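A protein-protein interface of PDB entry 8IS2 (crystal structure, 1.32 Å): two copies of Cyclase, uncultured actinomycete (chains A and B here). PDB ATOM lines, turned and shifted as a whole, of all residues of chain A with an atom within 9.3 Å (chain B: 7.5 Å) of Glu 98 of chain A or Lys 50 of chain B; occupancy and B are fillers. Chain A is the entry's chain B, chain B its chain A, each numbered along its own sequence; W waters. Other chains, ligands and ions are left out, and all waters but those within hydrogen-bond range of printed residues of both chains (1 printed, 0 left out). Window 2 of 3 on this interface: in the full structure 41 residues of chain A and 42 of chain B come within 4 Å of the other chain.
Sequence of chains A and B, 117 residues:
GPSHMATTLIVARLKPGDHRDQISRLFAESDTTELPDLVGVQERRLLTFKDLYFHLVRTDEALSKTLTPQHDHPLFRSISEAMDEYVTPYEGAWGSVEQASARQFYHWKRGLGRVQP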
ATOM      1  N   ILE A  10     -22.089   4.315  -8.837  1.00  0.00           N
ATOM      2  CA  ILE A  10     -20.957   5.105  -9.318  1.00  0.00           C
ATOM      3  C   ILE A  10     -20.104   4.234 -10.225  1.00  0.00           C
ATOM      4  O   ILE A  10     -19.861   3.055  -9.930  1.00  0.00           O
ATOM      5  CB  ILE A  10     -20.147   5.670  -8.135  1.00  0.00           C
ATOM      6  CG1 ILE A  10     -20.980   6.718  -7.395  1.00  0.00           C
ATOM      7  CG2 ILE A  10     -18.838   6.268  -8.607  1.00  0.00           C
ATOM      8  CD1 ILE A  10     -20.374   7.187  -6.103  1.00  0.00           C
ATOM      9  N   VAL A  11     -19.653   4.811 -11.337  1.00  0.00           N
ATOM     10  CA  VAL A  11     -18.963   4.108 -12.408  1.00  0.00           C
ATOM     11  C   VAL A  11     -17.615   4.772 -12.611  1.00  0.00           C
ATOM     12  O   VAL A  11     -17.534   6.001 -12.706  1.00  0.00           O
ATOM     13  CB  VAL A  11     -19.773   4.193 -13.713  1.00  0.00           C
ATOM     14  CG1 VAL A  11     -19.050   3.469 -14.839  1.00  0.00           C
ATOM     15  CG2 VAL A  11     -21.189   3.652 -13.517  1.00  0.00           C
ATOM     16  N   ARG A  13     -13.466   3.774 -14.544  1.00  0.00           N
ATOM     17  CA  ARG A  13     -12.675   2.835 -15.319  1.00  0.00           C
ATOM     18  C   ARG A  13     -11.521   2.344 -14.464  1.00  0.00           C
ATOM     19  O   ARG A  13     -10.850   3.145 -13.803  1.00  0.00           O
ATOM     20  CB  ARG A  13     -12.125   3.483 -16.579  1.00  0.00           C
ATOM     21  CG  ARG A  13     -11.620   2.447 -17.551  1.00  0.00           C
ATOM     22  CD  ARG A  13     -11.239   3.029 -18.884  1.00  0.00           C
ATOM     23  NE  ARG A  13     -12.316   3.821 -19.467  1.00  0.00           N
ATOM     24  CZ  ARG A  13     -13.201   3.356 -20.340  1.00  0.00           C
ATOM     25  NH1 ARG A  13     -13.246   2.073 -20.660  1.00  0.00           N
ATOM     26  NH2 ARG A  13     -14.051   4.203 -20.914  1.00  0.00           N
ATOM     27  N   PRO A  89     -11.491   8.414 -14.391  1.00  0.00           N
ATOM     28  CA  PRO A  89     -12.855   8.698 -14.858  1.00  0.00           C
ATOM     29  C   PRO A  89     -13.187   7.941 -16.141  1.00  0.00           C
ATOM     30  O   PRO A  89     -12.348   7.773 -17.024  1.00  0.00           O
ATOM     31  CB  PRO A  89     -12.829  10.213 -15.082  1.00  0.00           C
ATOM     32  CG  PRO A  89     -11.815  10.696 -14.081  1.00  0.00           C
ATOM     33  CD  PRO A  89     -10.734   9.652 -14.119  1.00  0.00           C
ATOM     34  N   TYR A  90     -14.426   7.459 -16.229  1.00  0.00           N
ATOM     35  CA  TYR A  90     -14.849   6.725 -17.420  1.00  0.00           C
ATOM     36  C   TYR A  90     -14.727   7.568 -18.687  1.00  0.00           C
ATOM     37  O   TYR A  90     -14.294   7.070 -19.731  1.00  0.00           O
ATOM     38  CB  TYR A  90     -16.273   6.198 -17.231  1.00  0.00           C
ATOM     39  CG  TYR A  90     -16.839   5.456 -18.430  1.00  0.00           C
ATOM     40  CD1 TYR A  90     -16.420   4.167 -18.736  1.00  0.00           C
ATOM     41  CD2 TYR A  90     -17.791   6.046 -19.258  1.00  0.00           C
ATOM     42  CE1 TYR A  90     -16.942   3.477 -19.828  1.00  0.00           C
ATOM     43  CE2 TYR A  90     -18.310   5.361 -20.359  1.00  0.00           C
ATOM     44  CZ  TYR A  90     -17.875   4.086 -20.636  1.00  0.00           C
ATOM     45  OH  TYR A  90     -18.392   3.420 -21.721  1.00  0.00           O
ATOM     46  N   GLU A  91     -15.081   8.846 -18.615  1.00  0.00           N
ATOM     47  CA  GLU A  91     -14.897   9.790 -19.710  1.00  0.00           C
ATOM     48  C   GLU A  91     -14.037  10.947 -19.220  1.00  0.00           C
ATOM     49  O   GLU A  91     -14.303  11.517 -18.156  1.00  0.00           O
ATOM     50  CB  GLU A  91     -16.239  10.303 -20.229  1.00  0.00           C
ATOM     51  CG  GLU A  91     -16.710   9.596 -21.482  1.00  0.00           C
ATOM     52  CD  GLU A  91     -15.889   9.972 -22.708  1.00  0.00           C
ATOM     53  OE1 GLU A  91     -16.007  11.128 -23.180  1.00  0.00           O
ATOM     54  OE2 GLU A  91     -15.116   9.115 -23.196  1.00  0.00           O
ATOM     55  N   GLY A  92     -13.013  11.298 -20.008  1.00  0.00           N
ATOM     56  CA  GLY A  92     -12.010  12.231 -19.539  1.00  0.00           C
ATOM     57  C   GLY A  92     -12.335  13.688 -19.768  1.00  0.00           C
ATOM     58  O   GLY A  92     -11.801  14.547 -19.066  1.00  0.00           O
ATOM     59  N   ALA A  93     -13.227  13.998 -20.716  1.00  0.00           N
ATOM     60  CA  ALA A  93     -13.396  15.385 -21.153  1.00  0.00           C
ATOM     61  C   ALA A  93     -13.748  16.317 -19.995  1.00  0.00           C
ATOM     62  O   ALA A  93     -13.179  17.410 -19.867  1.00  0.00           O
ATOM     63  CB  ALA A  93     -14.454  15.474 -22.254  1.00  0.00           C
ATOM     64  N   TRP A  94     -14.701  15.903 -19.161  1.00  0.00           N
ATOM     65  CA  TRP A  94     -15.068  16.568 -17.917  1.00  0.00           C
ATOM     66  C   TRP A  94     -14.831  15.645 -16.723  1.00  0.00           C
ATOM     67  O   TRP A  94     -15.519  15.730 -15.701  1.00  0.00           O
ATOM     68  CB  TRP A  94     -16.510  17.083 -17.966  1.00  0.00           C
ATOM     69  CG  TRP A  94     -16.733  18.180 -18.976  1.00  0.00           C
ATOM     70  CD1 TRP A  94     -17.324  18.060 -20.208  1.00  0.00           C
ATOM     71  CD2 TRP A  94     -16.373  19.561 -18.843  1.00  0.00           C
ATOM     72  NE1 TRP A  94     -17.357  19.269 -20.838  1.00  0.00           N
ATOM     73  CE2 TRP A  94     -16.780  20.211 -20.030  1.00  0.00           C
ATOM     74  CE3 TRP A  94     -15.754  20.316 -17.838  1.00  0.00           C
ATOM     75  CZ2 TRP A  94     -16.584  21.577 -20.238  1.00  0.00           C
ATOM     76  CZ3 TRP A  94     -15.556  21.664 -18.049  1.00  0.00           C
ATOM     77  CH2 TRP A  94     -15.977  22.284 -19.240  1.00  0.00           C
ATOM     78  N   GLY A  95     -13.831  14.771 -16.848  1.00  0.00           N
ATOM     79  CA  GLY A  95     -13.547  13.815 -15.792  1.00  0.00           C
ATOM     80  C   GLY A  95     -13.308  14.486 -14.449  1.00  0.00           C
ATOM     81  O   GLY A  95     -12.634  15.517 -14.358  1.00  0.00           O
ATOM     82  N   SER A  96     -13.918  13.909 -13.408  1.00  0.00           N
ATOM     83  CA  SER A  96     -13.772  14.295 -12.002  1.00  0.00           C
ATOM     84  C   SER A  96     -14.705  15.426 -11.579  1.00  0.00           C
ATOM     85  O   SER A  96     -14.950  15.606 -10.384  1.00  0.00           O
ATOM     86  CB  SER A  96     -12.320  14.617 -11.618  1.00  0.00           C
ATOM     87  OG  SER A  96     -11.485  13.479 -11.655  1.00  0.00           O
ATOM     88  N   VAL A  97     -15.239  16.189 -12.523  1.00  0.00           N
ATOM     89  CA  VAL A  97     -16.115  17.299 -12.172  1.00  0.00           C
ATOM     90  C   VAL A  97     -17.542  17.104 -12.641  1.00  0.00           C
ATOM     91  O   VAL A  97     -18.439  17.785 -12.128  1.00  0.00           O
ATOM     92  CB  VAL A  97     -15.567  18.653 -12.659  1.00  0.00           C
ATOM     93  CG1 VAL A  97     -14.142  18.845 -12.148  1.00  0.00           C
ATOM     94  CG2 VAL A  97     -15.642  18.741 -14.159  1.00  0.00           C
ATOM     95  N   GLU A  98     -17.797  16.226 -13.599  1.00  0.00           N
ATOM     96  CA  GLU A  98     -19.164  15.838 -13.876  1.00  0.00           C
ATOM     97  C   GLU A  98     -19.488  14.606 -13.052  1.00  0.00           C
ATOM     98  O   GLU A  98     -18.598  13.864 -12.623  1.00  0.00           O
ATOM     99  CB  GLU A  98     -19.373  15.573 -15.364  1.00  0.00           C
ATOM    100  CG  GLU A  98     -18.719  14.318 -15.876  1.00  0.00           C
ATOM    101  CD  GLU A  98     -18.908  14.141 -17.370  1.00  0.00           C
ATOM    102  OE1 GLU A  98     -19.848  14.738 -17.938  1.00  0.00           O
ATOM    103  OE2 GLU A  98     -18.107  13.410 -17.980  1.00  0.00           O
ATOM    104  N   GLN A  99     -20.778  14.401 -12.809  1.00  0.00           N
ATOM    105  CA  GLN A  99     -21.188  13.294 -11.965  1.00  0.00           C
ATOM    106  C   GLN A  99     -20.772  11.964 -12.582  1.00  0.00           C
ATOM    107  O   GLN A  99     -20.844  11.766 -13.802  1.00  0.00           O
ATOM    108  CB  GLN A  99     -22.696  13.343 -11.718  1.00  0.00           C
ATOM    109  CG  GLN A  99     -23.547  12.589 -12.725  1.00  0.00           C
ATOM    110  CD  GLN A  99     -25.037  12.798 -12.517  1.00  0.00           C
ATOM    111  OE1 GLN A  99     -25.506  13.931 -12.405  1.00  0.00           O
ATOM    112  NE2 GLN A  99     -25.790  11.705 -12.476  1.00  0.00           N
ATOM    113  N   ALA A 100     -20.312  11.056 -11.721  1.00  0.00           N
ATOM    114  CA  ALA A 100     -19.942   9.698 -12.086  1.00  0.00           C
ATOM    115  C   ALA A 100     -21.013   8.679 -11.698  1.00  0.00           C
ATOM    116  O   ALA A 100     -20.770   7.467 -11.762  1.00  0.00           O
ATOM    117  CB  ALA A 100     -18.592   9.346 -11.448  1.00  0.00           C
ATOM    118  N   SER A 101     -22.190   9.142 -11.284  1.00  0.00           N
ATOM    119  CA  SER A 101     -23.265   8.253 -10.877  1.00  0.00           C
ATOM    120  C   SER A 101     -24.266   8.071 -12.007  1.00  0.00           C
ATOM    121  O   SER A 101     -24.614   9.024 -12.710  1.00  0.00           O
ATOM    122  CB  SER A 101     -23.983   8.798  -9.646  1.00  0.00           C
ATOM    123  OG  SER A 101     -24.511  10.084  -9.900  1.00  0.00           O
ATOM    124  N   ALA A 102     -24.731   6.832 -12.159  1.00  0.00           N
ATOM    125  CA  ALA A 102     -25.733   6.496 -13.150  1.00  0.00           C
ATOM    126  C   ALA A 102     -27.071   7.126 -12.774  1.00  0.00           C
ATOM    127  O   ALA A 102     -27.283   7.551 -11.639  1.00  0.00           O
ATOM    128  CB  ALA A 102     -25.892   4.979 -13.210  1.00  0.00           C
ATOM    129  N   ARG A 103     -27.969   7.209 -13.757  1.00  0.00           N
ATOM    130  CA  ARG A 103     -29.305   7.763 -13.563  1.00  0.00           C
ATOM    131  C   ARG A 103     -30.328   6.648 -13.740  1.00  0.00           C
ATOM    132  O   ARG A 103     -30.398   6.019 -14.802  1.00  0.00           O
ATOM    133  CB  ARG A 103     -29.571   8.917 -14.532  1.00  0.00           C
ATOM    134  CG  ARG A 103     -28.826  10.201 -14.183  1.00  0.00           C
ATOM    135  CD  ARG A 103     -29.785  11.374 -13.960  1.00  0.00           C
ATOM    136  NE  ARG A 103     -30.564  11.708 -15.151  1.00  0.00           N
ATOM    137  CZ  ARG A 103     -31.340  12.779 -15.269  1.00  0.00           C
ATOM    138  NH1 ARG A 103     -31.462  13.662 -14.291  1.00  0.00           N
ATOM    139  NH2 ARG A 103     -32.009  12.974 -16.404  1.00  0.00           N
ATOM    140  N   LEU B  14     -25.151   0.979 -24.641  1.00  0.00           N
ATOM    141  CA  LEU B  14     -26.268   1.507 -25.416  1.00  0.00           C
ATOM    142  C   LEU B  14     -25.839   1.799 -26.847  1.00  0.00           C
ATOM    143  O   LEU B  14     -24.713   2.242 -27.097  1.00  0.00           O
ATOM    144  CB  LEU B  14     -26.774   2.803 -24.779  1.00  0.00           C
ATOM    145  CG  LEU B  14     -27.418   2.683 -23.398  1.00  0.00           C
ATOM    146  CD1 LEU B  14     -27.446   4.022 -22.671  1.00  0.00           C
ATOM    147  CD2 LEU B  14     -28.819   2.103 -23.531  1.00  0.00           C
ATOM    148  N   GLY B  17     -28.402   7.121 -29.633  1.00  0.00           N
ATOM    149  CA  GLY B  17     -29.757   7.596 -29.441  1.00  0.00           C
ATOM    150  C   GLY B  17     -30.121   7.655 -27.972  1.00  0.00           C
ATOM    151  O   GLY B  17     -29.283   7.479 -27.082  1.00  0.00           O
ATOM    152  N   THR B  48     -28.774   4.209 -16.581  1.00  0.00           N
ATOM    153  CA  THR B  48     -27.827   4.499 -17.636  1.00  0.00           C
ATOM    154  C   THR B  48     -26.754   5.422 -17.090  1.00  0.00           C
ATOM    155  O   THR B  48     -26.990   6.202 -16.159  1.00  0.00           O
ATOM    156  CB  THR B  48     -28.455   5.174 -18.855  1.00  0.00           C
ATOM    157  OG1 THR B  48     -28.891   6.494 -18.524  1.00  0.00           O
ATOM    158  CG2 THR B  48     -29.635   4.388 -19.359  1.00  0.00           C
ATOM    159  N   PHE B  49     -25.562   5.289 -17.649  1.00  0.00           N
ATOM    160  CA  PHE B  49     -24.471   6.232 -17.425  1.00  0.00           C
ATOM    161  C   PHE B  49     -23.716   6.362 -18.738  1.00  0.00           C
ATOM    162  O   PHE B  49     -23.110   5.388 -19.199  1.00  0.00           O
ATOM    163  CB  PHE B  49     -23.529   5.752 -16.328  1.00  0.00           C
ATOM    164  CG  PHE B  49     -22.378   6.694 -16.070  1.00  0.00           C
ATOM    165  CD1 PHE B  49     -22.585   7.903 -15.421  1.00  0.00           C
ATOM    166  CD2 PHE B  49     -21.085   6.374 -16.482  1.00  0.00           C
ATOM    167  CE1 PHE B  49     -21.558   8.766 -15.208  1.00  0.00           C
ATOM    168  CE2 PHE B  49     -20.041   7.249 -16.251  1.00  0.00           C
ATOM    169  CZ  PHE B  49     -20.286   8.444 -15.618  1.00  0.00           C
ATOM    170  N   LYS B  50     -23.783   7.533 -19.361  1.00  0.00           N
ATOM    171  CA  LYS B  50     -23.100   7.777 -20.636  1.00  0.00           C
ATOM    172  C   LYS B  50     -23.609   6.753 -21.645  1.00  0.00           C
ATOM    173  O   LYS B  50     -24.831   6.662 -21.844  1.00  0.00           O
ATOM    174  CB  LYS B  50     -21.578   7.821 -20.447  1.00  0.00           C
ATOM    175  CG  LYS B  50     -21.076   8.772 -19.369  1.00  0.00           C
ATOM    176  CD  LYS B  50     -20.941  10.179 -19.875  1.00  0.00           C
ATOM    177  CE  LYS B  50     -20.089  10.998 -18.922  1.00  0.00           C
ATOM    178  NZ  LYS B  50     -20.656  11.080 -17.544  1.00  0.00           N
ATOM    179  N   ASP B  51     -22.746   5.953 -22.267  1.00  0.00           N
ATOM    180  CA  ASP B  51     -23.184   4.925 -23.197  1.00  0.00           C
ATOM    181  C   ASP B  51     -23.343   3.551 -22.543  1.00  0.00           C
ATOM    182  O   ASP B  51     -23.282   2.545 -23.246  1.00  0.00           O
ATOM    183  CB  ASP B  51     -22.232   4.839 -24.391  1.00  0.00           C
ATOM    184  CG  ASP B  51     -20.812   4.468 -23.992  1.00  0.00           C
ATOM    185  OD1 ASP B  51     -20.479   4.588 -22.792  1.00  0.00           O
ATOM    186  OD2 ASP B  51     -20.031   4.060 -24.880  1.00  0.00           O
ATOM    187  N   LEU B  52     -23.520   3.483 -21.224  1.00  0.00           N
ATOM    188  CA  LEU B  52     -23.660   2.221 -20.508  1.00  0.00           C
ATOM    189  C   LEU B  52     -25.094   2.037 -20.041  1.00  0.00           C
ATOM    190  O   LEU B  52     -25.725   2.983 -19.558  1.00  0.00           O
ATOM    191  CB  LEU B  52     -22.735   2.169 -19.290  1.00  0.00           C
ATOM    192  CG  LEU B  52     -21.234   2.224 -19.561  1.00  0.00           C
ATOM    193  CD1 LEU B  52     -20.475   2.267 -18.241  1.00  0.00           C
ATOM    194  CD2 LEU B  52     -20.791   1.055 -20.432  1.00  0.00           C
ATOM    195  N   TYR B  53     -25.590   0.814 -20.189  1.00  0.00           N
ATOM    196  CA  TYR B  53     -26.881   0.357 -19.697  1.00  0.00           C
ATOM    197  C   TYR B  53     -26.665  -0.574 -18.508  1.00  0.00           C
ATOM    198  O   TYR B  53     -25.771  -1.422 -18.532  1.00  0.00           O
ATOM    199  CB  TYR B  53     -27.603  -0.397 -20.815  1.00  0.00           C
ATOM    200  CG  TYR B  53     -28.706  -1.332 -20.374  1.00  0.00           C
ATOM    201  CD1 TYR B  53     -29.978  -0.856 -20.086  1.00  0.00           C
ATOM    202  CD2 TYR B  53     -28.484  -2.713 -20.271  1.00  0.00           C
ATOM    203  CE1 TYR B  53     -30.977  -1.708 -19.713  1.00  0.00           C
ATOM    204  CE2 TYR B  53     -29.484  -3.569 -19.886  1.00  0.00           C
ATOM    205  CZ  TYR B  53     -30.725  -3.061 -19.612  1.00  0.00           C
ATOM    206  OH  TYR B  53     -31.713  -3.916 -19.243  1.00  0.00           O
ATOM    207  N   PHE B  54     -27.493  -0.420 -17.473  1.00  0.00           N
ATOM    208  CA  PHE B  54     -27.396  -1.246 -16.274  1.00  0.00           C
ATOM    209  C   PHE B  54     -28.751  -1.828 -15.924  1.00  0.00           C
ATOM    210  O   PHE B  54     -29.745  -1.103 -15.888  1.00  0.00           O
ATOM    211  CB  PHE B  54     -26.879  -0.473 -15.063  1.00  0.00           C
ATOM    212  CG  PHE B  54     -25.525   0.128 -15.260  1.00  0.00           C
ATOM    213  CD1 PHE B  54     -24.406  -0.668 -15.180  1.00  0.00           C
ATOM    214  CD2 PHE B  54     -25.367   1.470 -15.554  1.00  0.00           C
ATOM    215  CE1 PHE B  54     -23.151  -0.135 -15.368  1.00  0.00           C
ATOM    216  CE2 PHE B  54     -24.118   2.006 -15.741  1.00  0.00           C
ATOM    217  CZ  PHE B  54     -23.004   1.198 -15.653  1.00  0.00           C
HETATM  218  O   HOH W   1     -31.513   7.017 -17.182  1.00  0.00           O
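The backbone NH of Arg 103 of chain A sits at hydrogen-bond distance from the backbone carbonyl oxygen of Thr 48 of chain B (2.8 Å). The side-chain carboxylate (OD1) of Asp 51 of chain B lies within hydrogen-bond range of the side-chain hydroxyl (OH) of Tyr 90 of chain A, 2.6 Å away. The side-chain carboxylate (OE2) of Glu 98 of chain A is in salt-bridge range of the side-chain amino group (NZ) of Lys 50 of chain B, at 3.5 Å.
The guanidinium group (NH2) of Arg 13 of chain A is in hydrogen-bond range of the backbone carbonyl oxygen (O) of Tyr 90 of chain A, at 3.1 Å. The backbone carbonyl oxygen (O) of Ser 101 of chain A sits at hydrogen-bond distance from the side-chain amide nitrogen (NE2) of Gln 99 of chain A, at 2.9 Å. O of Asp 51 of chain B is in hydrogen-bond range of N of Leu 14 of chain B (2.8 Å). The backbone carbonyl oxygen (O) of Ala 100 of chain A is in hydrogen-bond range of the backbone NH (N) of Val 11 of chain A (2.9 Å).
Among the printed residues, merely in contact across the chains: Val 11 of chain A with Phe 49 of chain B, Val 11 of chain A with Leu 52 of chain B, Val 11 of chain A with Phe 54 of chain B, Tyr 90 of chain A with Phe 49 of chain B, Tyr 90 of chain A with Leu 52 of chain B, Gln 99 of chain A with Phe 49 of chain B, Gln 99 of chain A with Lys 50 of chain B, Ala 100 of chain A with Phe 49 of chain B, Ser 101 of chain A with Phe 49 of chain B, Ala 102 of chain A with Thr 48 of chain B and Ala 102 of chain A with Phe 49 of chain B.
Of the printed residues of chain B, Glu 98 of chain A touches Lys 50 (3.3 Å). Of chain A, only Glu 98 (3.3 Å) and Gln 99 (3.8 Å) come within 4 Å of Lys 50 of chain B. Of the printed residues of chain B, Ser 101 of chain A touches Phe 49. Of the printed residues of chain B, Val 11 of chain A touches Phe 49 (3.8 Å), Leu 52 (3.9 Å) and Phe 54 (3.7 Å). Printed residues of chain B within 4 Å of Ala 102 of chain A: Thr 48 (3.3 Å) and Phe 49 (3.9 Å). The nearest printed residue of chain B that does not touch Ala 102 of chain A is Phe 54 of chain B (4.3 Å).
Hydrophobic or aromatic side chains of chain B within 4 Å of the printed part of chain A: Phe 49, Leu 52 and Phe 54. Among the printed residues, Asp or Glu carboxylates within 4 Å of a Lys or Arg side-chain nitrogen of the other chain: Glu 98 of chain A with Lys 50 of chain B (3.5 Å).
No position is printed for both chains.
Water W1 bridges O of Arg 103 of chain A and OG1 of Thr 48 of chain B.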
